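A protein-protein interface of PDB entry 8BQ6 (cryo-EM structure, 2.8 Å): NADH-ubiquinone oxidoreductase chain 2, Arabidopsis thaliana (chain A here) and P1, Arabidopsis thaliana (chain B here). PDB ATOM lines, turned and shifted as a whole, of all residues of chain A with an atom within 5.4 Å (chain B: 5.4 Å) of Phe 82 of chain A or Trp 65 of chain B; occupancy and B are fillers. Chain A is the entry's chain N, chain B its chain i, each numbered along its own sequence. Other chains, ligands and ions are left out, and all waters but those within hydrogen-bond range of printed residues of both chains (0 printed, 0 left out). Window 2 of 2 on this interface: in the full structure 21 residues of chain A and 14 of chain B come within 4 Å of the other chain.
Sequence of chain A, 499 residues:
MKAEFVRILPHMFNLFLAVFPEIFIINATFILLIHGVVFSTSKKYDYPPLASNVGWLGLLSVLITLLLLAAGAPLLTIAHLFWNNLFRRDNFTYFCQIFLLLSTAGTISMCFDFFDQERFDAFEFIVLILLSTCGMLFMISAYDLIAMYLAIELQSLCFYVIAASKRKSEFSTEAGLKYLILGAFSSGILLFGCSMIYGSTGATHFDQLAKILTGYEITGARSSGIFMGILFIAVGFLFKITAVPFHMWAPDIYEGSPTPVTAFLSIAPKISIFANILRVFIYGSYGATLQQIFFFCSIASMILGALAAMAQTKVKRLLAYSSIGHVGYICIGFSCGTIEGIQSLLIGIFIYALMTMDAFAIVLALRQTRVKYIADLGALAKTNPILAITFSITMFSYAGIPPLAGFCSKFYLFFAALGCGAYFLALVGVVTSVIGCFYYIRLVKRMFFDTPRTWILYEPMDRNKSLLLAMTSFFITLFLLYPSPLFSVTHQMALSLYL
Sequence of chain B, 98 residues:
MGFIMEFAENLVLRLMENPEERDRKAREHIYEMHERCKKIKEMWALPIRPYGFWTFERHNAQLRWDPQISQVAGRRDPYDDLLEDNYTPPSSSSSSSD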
ATOM      1  N   MET A  12      23.538  27.992 -16.705  1.00  0.00           N
ATOM      2  CA  MET A  12      22.165  28.417 -17.113  1.00  0.00           C
ATOM      3  C   MET A  12      22.177  29.880 -17.575  1.00  0.00           C
ATOM      4  O   MET A  12      21.665  30.143 -18.666  1.00  0.00           O
ATOM      5  CB  MET A  12      21.162  28.244 -15.968  1.00  0.00           C
ATOM      6  CG  MET A  12      19.727  28.587 -16.335  1.00  0.00           C
ATOM      7  SD  MET A  12      19.031  27.566 -17.662  1.00  0.00           S
ATOM      8  CE  MET A  12      18.280  26.246 -16.709  1.00  0.00           C
ATOM      9  N   LEU A  15      23.572  30.721 -21.118  1.00  0.00           N
ATOM     10  CA  LEU A  15      22.761  30.439 -22.297  1.00  0.00           C
ATOM     11  C   LEU A  15      22.094  31.699 -22.827  1.00  0.00           C
ATOM     12  O   LEU A  15      22.004  31.890 -24.043  1.00  0.00           O
ATOM     13  CB  LEU A  15      21.699  29.389 -21.981  1.00  0.00           C
ATOM     14  CG  LEU A  15      22.114  28.081 -21.315  1.00  0.00           C
ATOM     15  CD1 LEU A  15      20.877  27.376 -20.826  1.00  0.00           C
ATOM     16  CD2 LEU A  15      22.881  27.193 -22.274  1.00  0.00           C
ATOM     17  N   ALA A  79      24.897  28.347 -27.421  1.00  0.00           N
ATOM     18  CA  ALA A  79      23.763  27.502 -27.050  1.00  0.00           C
ATOM     19  C   ALA A  79      22.780  27.339 -28.205  1.00  0.00           C
ATOM     20  O   ALA A  79      21.563  27.371 -28.015  1.00  0.00           O
ATOM     21  CB  ALA A  79      23.054  28.052 -25.811  1.00  0.00           C
ATOM     22  N   HIS A  80      23.307  27.164 -29.419  1.00  0.00           N
ATOM     23  CA  HIS A  80      22.436  27.138 -30.587  1.00  0.00           C
ATOM     24  C   HIS A  80      21.513  25.925 -30.589  1.00  0.00           C
ATOM     25  O   HIS A  80      20.422  25.990 -31.165  1.00  0.00           O
ATOM     26  CB  HIS A  80      23.266  27.183 -31.871  1.00  0.00           C
ATOM     27  CG  HIS A  80      24.020  25.923 -32.151  1.00  0.00           C
ATOM     28  ND1 HIS A  80      24.921  25.378 -31.261  1.00  0.00           N
ATOM     29  CD2 HIS A  80      24.025  25.110 -33.235  1.00  0.00           C
ATOM     30  CE1 HIS A  80      25.436  24.278 -31.778  1.00  0.00           C
ATOM     31  NE2 HIS A  80      24.910  24.093 -32.974  1.00  0.00           N
ATOM     32  N   LEU A  81      21.917  24.817 -29.963  1.00  0.00           N
ATOM     33  CA  LEU A  81      21.035  23.653 -29.906  1.00  0.00           C
ATOM     34  C   LEU A  81      19.911  23.854 -28.897  1.00  0.00           C
ATOM     35  O   LEU A  81      18.770  23.448 -29.142  1.00  0.00           O
ATOM     36  CB  LEU A  81      21.825  22.390 -29.567  1.00  0.00           C
ATOM     37  CG  LEU A  81      22.943  21.940 -30.506  1.00  0.00           C
ATOM     38  CD1 LEU A  81      23.472  20.590 -30.048  1.00  0.00           C
ATOM     39  CD2 LEU A  81      22.455  21.871 -31.943  1.00  0.00           C
ATOM     40  N   PHE A  82      20.214  24.446 -27.746  1.00  0.00           N
ATOM     41  CA  PHE A  82      19.159  24.740 -26.740  1.00  0.00           C
ATOM     42  C   PHE A  82      18.153  25.730 -27.332  1.00  0.00           C
ATOM     43  O   PHE A  82      16.946  25.526 -27.145  1.00  0.00           O
ATOM     44  CB  PHE A  82      19.806  25.248 -25.451  1.00  0.00           C
ATOM     45  CG  PHE A  82      18.866  25.834 -24.427  1.00  0.00           C
ATOM     46  CD1 PHE A  82      18.237  25.022 -23.499  1.00  0.00           C
ATOM     47  CD2 PHE A  82      18.624  27.198 -24.380  1.00  0.00           C
ATOM     48  CE1 PHE A  82      17.379  25.560 -22.553  1.00  0.00           C
ATOM     49  CE2 PHE A  82      17.756  27.733 -23.441  1.00  0.00           C
ATOM     50  CZ  PHE A  82      17.139  26.913 -22.527  1.00  0.00           C
ATOM     51  N   TRP A  83      18.633  26.746 -28.046  1.00  0.00           N
ATOM     52  CA  TRP A  83      17.774  27.775 -28.608  1.00  0.00           C
ATOM     53  C   TRP A  83      17.212  27.394 -29.970  1.00  0.00           C
ATOM     54  O   TRP A  83      16.526  28.213 -30.588  1.00  0.00           O
ATOM     55  CB  TRP A  83      18.551  29.088 -28.739  1.00  0.00           C
ATOM     56  CG  TRP A  83      18.887  29.758 -27.440  1.00  0.00           C
ATOM     57  CD1 TRP A  83      20.134  29.980 -26.944  1.00  0.00           C
ATOM     58  CD2 TRP A  83      17.974  30.324 -26.493  1.00  0.00           C
ATOM     59  NE1 TRP A  83      20.059  30.630 -25.742  1.00  0.00           N
ATOM     60  CE2 TRP A  83      18.743  30.856 -25.441  1.00  0.00           C
ATOM     61  CE3 TRP A  83      16.583  30.424 -26.426  1.00  0.00           C
ATOM     62  CZ2 TRP A  83      18.170  31.478 -24.339  1.00  0.00           C
ATOM     63  CZ3 TRP A  83      16.016  31.045 -25.329  1.00  0.00           C
ATOM     64  CH2 TRP A  83      16.808  31.564 -24.302  1.00  0.00           C
ATOM     65  N   ASN A  84      17.493  26.182 -30.454  1.00  0.00           N
ATOM     66  CA  ASN A  84      17.210  25.857 -31.848  1.00  0.00           C
ATOM     67  C   ASN A  84      15.714  25.850 -32.138  1.00  0.00           C
ATOM     68  O   ASN A  84      15.274  26.358 -33.174  1.00  0.00           O
ATOM     69  CB  ASN A  84      17.842  24.513 -32.206  1.00  0.00           C
ATOM     70  CG  ASN A  84      17.379  23.991 -33.544  1.00  0.00           C
ATOM     71  OD1 ASN A  84      17.632  24.603 -34.579  1.00  0.00           O
ATOM     72  ND2 ASN A  84      16.712  22.847 -33.535  1.00  0.00           N
ATOM     73  N   ASN A  85      14.911  25.299 -31.235  1.00  0.00           N
ATOM     74  CA  ASN A  85      13.471  25.267 -31.453  1.00  0.00           C
ATOM     75  C   ASN A  85      12.795  26.618 -31.238  1.00  0.00           C
ATOM     76  O   ASN A  85      11.575  26.705 -31.409  1.00  0.00           O
ATOM     77  CB  ASN A  85      12.829  24.194 -30.569  1.00  0.00           C
ATOM     78  CG  ASN A  85      13.166  22.791 -31.034  1.00  0.00           C
ATOM     79  OD1 ASN A  85      13.620  21.952 -30.260  1.00  0.00           O
ATOM     80  ND2 ASN A  85      12.935  22.531 -32.310  1.00  0.00           N
ATOM     81  N   LEU A  86      13.540  27.670 -30.900  1.00  0.00           N
ATOM     82  CA  LEU A  86      12.973  29.004 -30.724  1.00  0.00           C
ATOM     83  C   LEU A  86      13.386  30.005 -31.790  1.00  0.00           C
ATOM     84  O   LEU A  86      12.544  30.776 -32.250  1.00  0.00           O
ATOM     85  CB  LEU A  86      13.345  29.574 -29.352  1.00  0.00           C
ATOM     86  CG  LEU A  86      12.721  28.876 -28.148  1.00  0.00           C
ATOM     87  CD1 LEU A  86      11.314  28.396 -28.498  1.00  0.00           C
ATOM     88  CD2 LEU A  86      13.585  27.742 -27.631  1.00  0.00           C
ATOM     89  N   ALA B  61      20.653  20.376 -36.507  1.00  0.00           N
ATOM     90  CA  ALA B  61      20.533  20.701 -35.091  1.00  0.00           C
ATOM     91  C   ALA B  61      19.643  19.700 -34.358  1.00  0.00           C
ATOM     92  O   ALA B  61      19.954  19.295 -33.233  1.00  0.00           O
ATOM     93  CB  ALA B  61      20.003  22.124 -34.926  1.00  0.00           C
ATOM     94  N   GLN B  62      18.521  19.320 -34.971  1.00  0.00           N
ATOM     95  CA  GLN B  62      17.564  18.383 -34.322  1.00  0.00           C
ATOM     96  C   GLN B  62      18.241  17.038 -34.026  1.00  0.00           C
ATOM     97  O   GLN B  62      18.006  16.494 -32.945  1.00  0.00           O
ATOM     98  CB  GLN B  62      16.340  18.212 -35.222  1.00  0.00           C
ATOM     99  CG  GLN B  62      15.398  17.102 -34.777  1.00  0.00           C
ATOM    100  CD  GLN B  62      14.021  17.203 -35.380  1.00  0.00           C
ATOM    101  OE1 GLN B  62      13.846  17.652 -36.509  1.00  0.00           O
ATOM    102  NE2 GLN B  62      13.024  16.771 -34.628  1.00  0.00           N
ATOM    103  N   LEU B  63      19.084  16.545 -34.935  1.00  0.00           N
ATOM    104  CA  LEU B  63      19.702  15.235 -34.763  1.00  0.00           C
ATOM    105  C   LEU B  63      20.648  15.183 -33.570  1.00  0.00           C
ATOM    106  O   LEU B  63      20.959  14.088 -33.090  1.00  0.00           O
ATOM    107  CB  LEU B  63      20.453  14.847 -36.032  1.00  0.00           C
ATOM    108  CG  LEU B  63      19.560  14.274 -37.128  1.00  0.00           C
ATOM    109  CD1 LEU B  63      20.301  14.215 -38.448  1.00  0.00           C
ATOM    110  CD2 LEU B  63      19.037  12.931 -36.718  1.00  0.00           C
ATOM    111  N   ARG B  64      21.119  16.329 -33.088  1.00  0.00           N
ATOM    112  CA  ARG B  64      22.001  16.347 -31.932  1.00  0.00           C
ATOM    113  C   ARG B  64      21.311  16.817 -30.662  1.00  0.00           C
ATOM    114  O   ARG B  64      21.772  16.485 -29.566  1.00  0.00           O
ATOM    115  CB  ARG B  64      23.218  17.234 -32.209  1.00  0.00           C
ATOM    116  CG  ARG B  64      23.662  17.190 -33.656  1.00  0.00           C
ATOM    117  CD  ARG B  64      25.154  17.431 -33.784  1.00  0.00           C
ATOM    118  NE  ARG B  64      25.542  18.787 -33.415  1.00  0.00           N
ATOM    119  CZ  ARG B  64      25.352  19.855 -34.178  1.00  0.00           C
ATOM    120  NH1 ARG B  64      24.777  19.762 -35.366  1.00  0.00           N
ATOM    121  NH2 ARG B  64      25.753  21.045 -33.740  1.00  0.00           N
ATOM    122  N   TRP B  65      20.211  17.558 -30.786  1.00  0.00           N
ATOM    123  CA  TRP B  65      19.512  18.046 -29.606  1.00  0.00           C
ATOM    124  C   TRP B  65      18.456  17.053 -29.140  1.00  0.00           C
ATOM    125  O   TRP B  65      18.328  16.792 -27.940  1.00  0.00           O
ATOM    126  CB  TRP B  65      18.889  19.410 -29.899  1.00  0.00           C
ATOM    127  CG  TRP B  65      17.935  19.866 -28.853  1.00  0.00           C
ATOM    128  CD1 TRP B  65      16.578  19.882 -28.939  1.00  0.00           C
ATOM    129  CD2 TRP B  65      18.262  20.379 -27.558  1.00  0.00           C
ATOM    130  NE1 TRP B  65      16.035  20.371 -27.778  1.00  0.00           N
ATOM    131  CE2 TRP B  65      17.050  20.685 -26.913  1.00  0.00           C
ATOM    132  CE3 TRP B  65      19.462  20.602 -26.878  1.00  0.00           C
ATOM    133  CZ2 TRP B  65      17.002  21.202 -25.626  1.00  0.00           C
ATOM    134  CZ3 TRP B  65      19.411  21.117 -25.599  1.00  0.00           C
ATOM    135  CH2 TRP B  65      18.192  21.412 -24.987  1.00  0.00           C
ATOM    136  N   ASP B  66      17.701  16.478 -30.075  1.00  0.00           N
ATOM    137  CA  ASP B  66      16.673  15.507 -29.707  1.00  0.00           C
ATOM    138  C   ASP B  66      17.190  14.329 -28.887  1.00  0.00           C
ATOM    139  O   ASP B  66      16.481  13.915 -27.956  1.00  0.00           O
ATOM    140  CB  ASP B  66      15.940  15.017 -30.965  1.00  0.00           C
ATOM    141  CG  ASP B  66      14.696  15.835 -31.263  1.00  0.00           C
ATOM    142  OD1 ASP B  66      14.462  16.834 -30.552  1.00  0.00           O
ATOM    143  OD2 ASP B  66      13.948  15.478 -32.194  1.00  0.00           O
ATOM    144  N   PRO B  67      18.358  13.735 -29.165  1.00  0.00           N
ATOM    145  CA  PRO B  67      18.856  12.681 -28.261  1.00  0.00           C
ATOM    146  C   PRO B  67      19.063  13.148 -26.831  1.00  0.00           C
ATOM    147  O   PRO B  67      18.934  12.340 -25.903  1.00  0.00           O
ATOM    148  CB  PRO B  67      20.181  12.245 -28.902  1.00  0.00           C
ATOM    149  CG  PRO B  67      20.171  12.764 -30.266  1.00  0.00           C
ATOM    150  CD  PRO B  67      19.172  13.854 -30.388  1.00  0.00           C
ATOM    151  N   GLN B  68      19.391  14.424 -26.622  1.00  0.00           N
ATOM    152  CA  GLN B  68      19.597  14.935 -25.273  1.00  0.00           C
ATOM    153  C   GLN B  68      18.299  15.032 -24.479  1.00  0.00           C
ATOM    154  O   GLN B  68      18.342  15.015 -23.245  1.00  0.00           O
ATOM    155  CB  GLN B  68      20.277  16.302 -25.332  1.00  0.00           C
ATOM    156  CG  GLN B  68      21.697  16.270 -25.855  1.00  0.00           C
ATOM    157  CD  GLN B  68      22.260  17.656 -26.061  1.00  0.00           C
ATOM    158  OE1 GLN B  68      22.378  18.434 -25.117  1.00  0.00           O
ATOM    159  NE2 GLN B  68      22.598  17.980 -27.303  1.00  0.00           N
ATOM    160  N   ILE B  69      17.152  15.141 -25.147  1.00  0.00           N
ATOM    161  CA  ILE B  69      15.860  15.175 -24.474  1.00  0.00           C
ATOM    162  C   ILE B  69      15.094  13.869 -24.674  1.00  0.00           C
ATOM    163  O   ILE B  69      13.897  13.812 -24.410  1.00  0.00           O
ATOM    164  CB  ILE B  69      15.009  16.370 -24.931  1.00  0.00           C
ATOM    165  CG1 ILE B  69      15.075  16.519 -26.455  1.00  0.00           C
ATOM    166  CG2 ILE B  69      15.420  17.640 -24.198  1.00  0.00           C
ATOM    167  CD1 ILE B  69      13.996  17.386 -27.035  1.00  0.00           C
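The backbone carbonyl oxygen (O) of Arg 64 of chain B lies within hydrogen-bond range of the side-chain amide nitrogen (NE2) of Gln 68 of chain B (2.8 Å).
Among the printed residues, pairs that only touch across the chains: Leu 81 of chain A with Ala 61 of chain B (3.8 Å), Leu 81 of chain A with Arg 64 of chain B (3.8 Å), Leu 81 of chain A with Trp 65 of chain B (3.5 Å), Leu 81 of chain A with Gln 68 of chain B (3.9 Å), Phe 82 of chain A with Trp 65 of chain B (3.8 Å), Asn 84 of chain A with Ala 61 of chain B (3.4 Å) and Asn 85 of chain A with Trp 65 of chain B (3.8 Å).
Of chain B, only Trp 65 comes within 4 Å of Phe 82 of chain A. Trp 65 of chain B touches just these residues of chain A: Leu 81 (3.5 Å), Phe 82 (3.8 Å) and Asn 85 (3.8 Å). Of the printed residues of chain A, Arg 64 of chain B touches His 80 (3.3 Å) and Leu 81 (3.8 Å). Of the printed residues of chain A, Ala 61 of chain B touches Leu 81 (3.8 Å) and Asn 84 (3.4 Å). Leu 63 of chain B touches none of the printed residues of chain A. The nearest printed residue of chain B that does not touch Phe 82 of chain A is Gln 68 of chain B (6.9 Å). The nearest printed residue of chain A that does not touch Trp 65 of chain B is Asn 84 of chain A (5.5 Å). The nearest printed residue of chain B that does not touch Leu 81 of chain A is Gln 62 of chain B (5.6 Å).
NH2 of Arg 64 of chain B sits at hydrogen-bond distance from NE2 of His 80 of chain A (3.3 Å).
Of the 9 printed residues of chain B, 4 touch a printed residue of chain A. Printed residues of chain B that touch a printed residue of chain A: Ala 61, Arg 64, Trp 65 and Gln 68. Of the 10 printed residues of chain A, 5 touch a printed residue of chain B. Printed residues of chain A that touch a printed residue of chain B: His 80, Leu 81, Phe 82, Asn 84 and Asn 85. Among the printed residues, no Asp or Glu carboxylate lies within 4 Å of a Lys or Arg side-chain nitrogen of the other chain.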
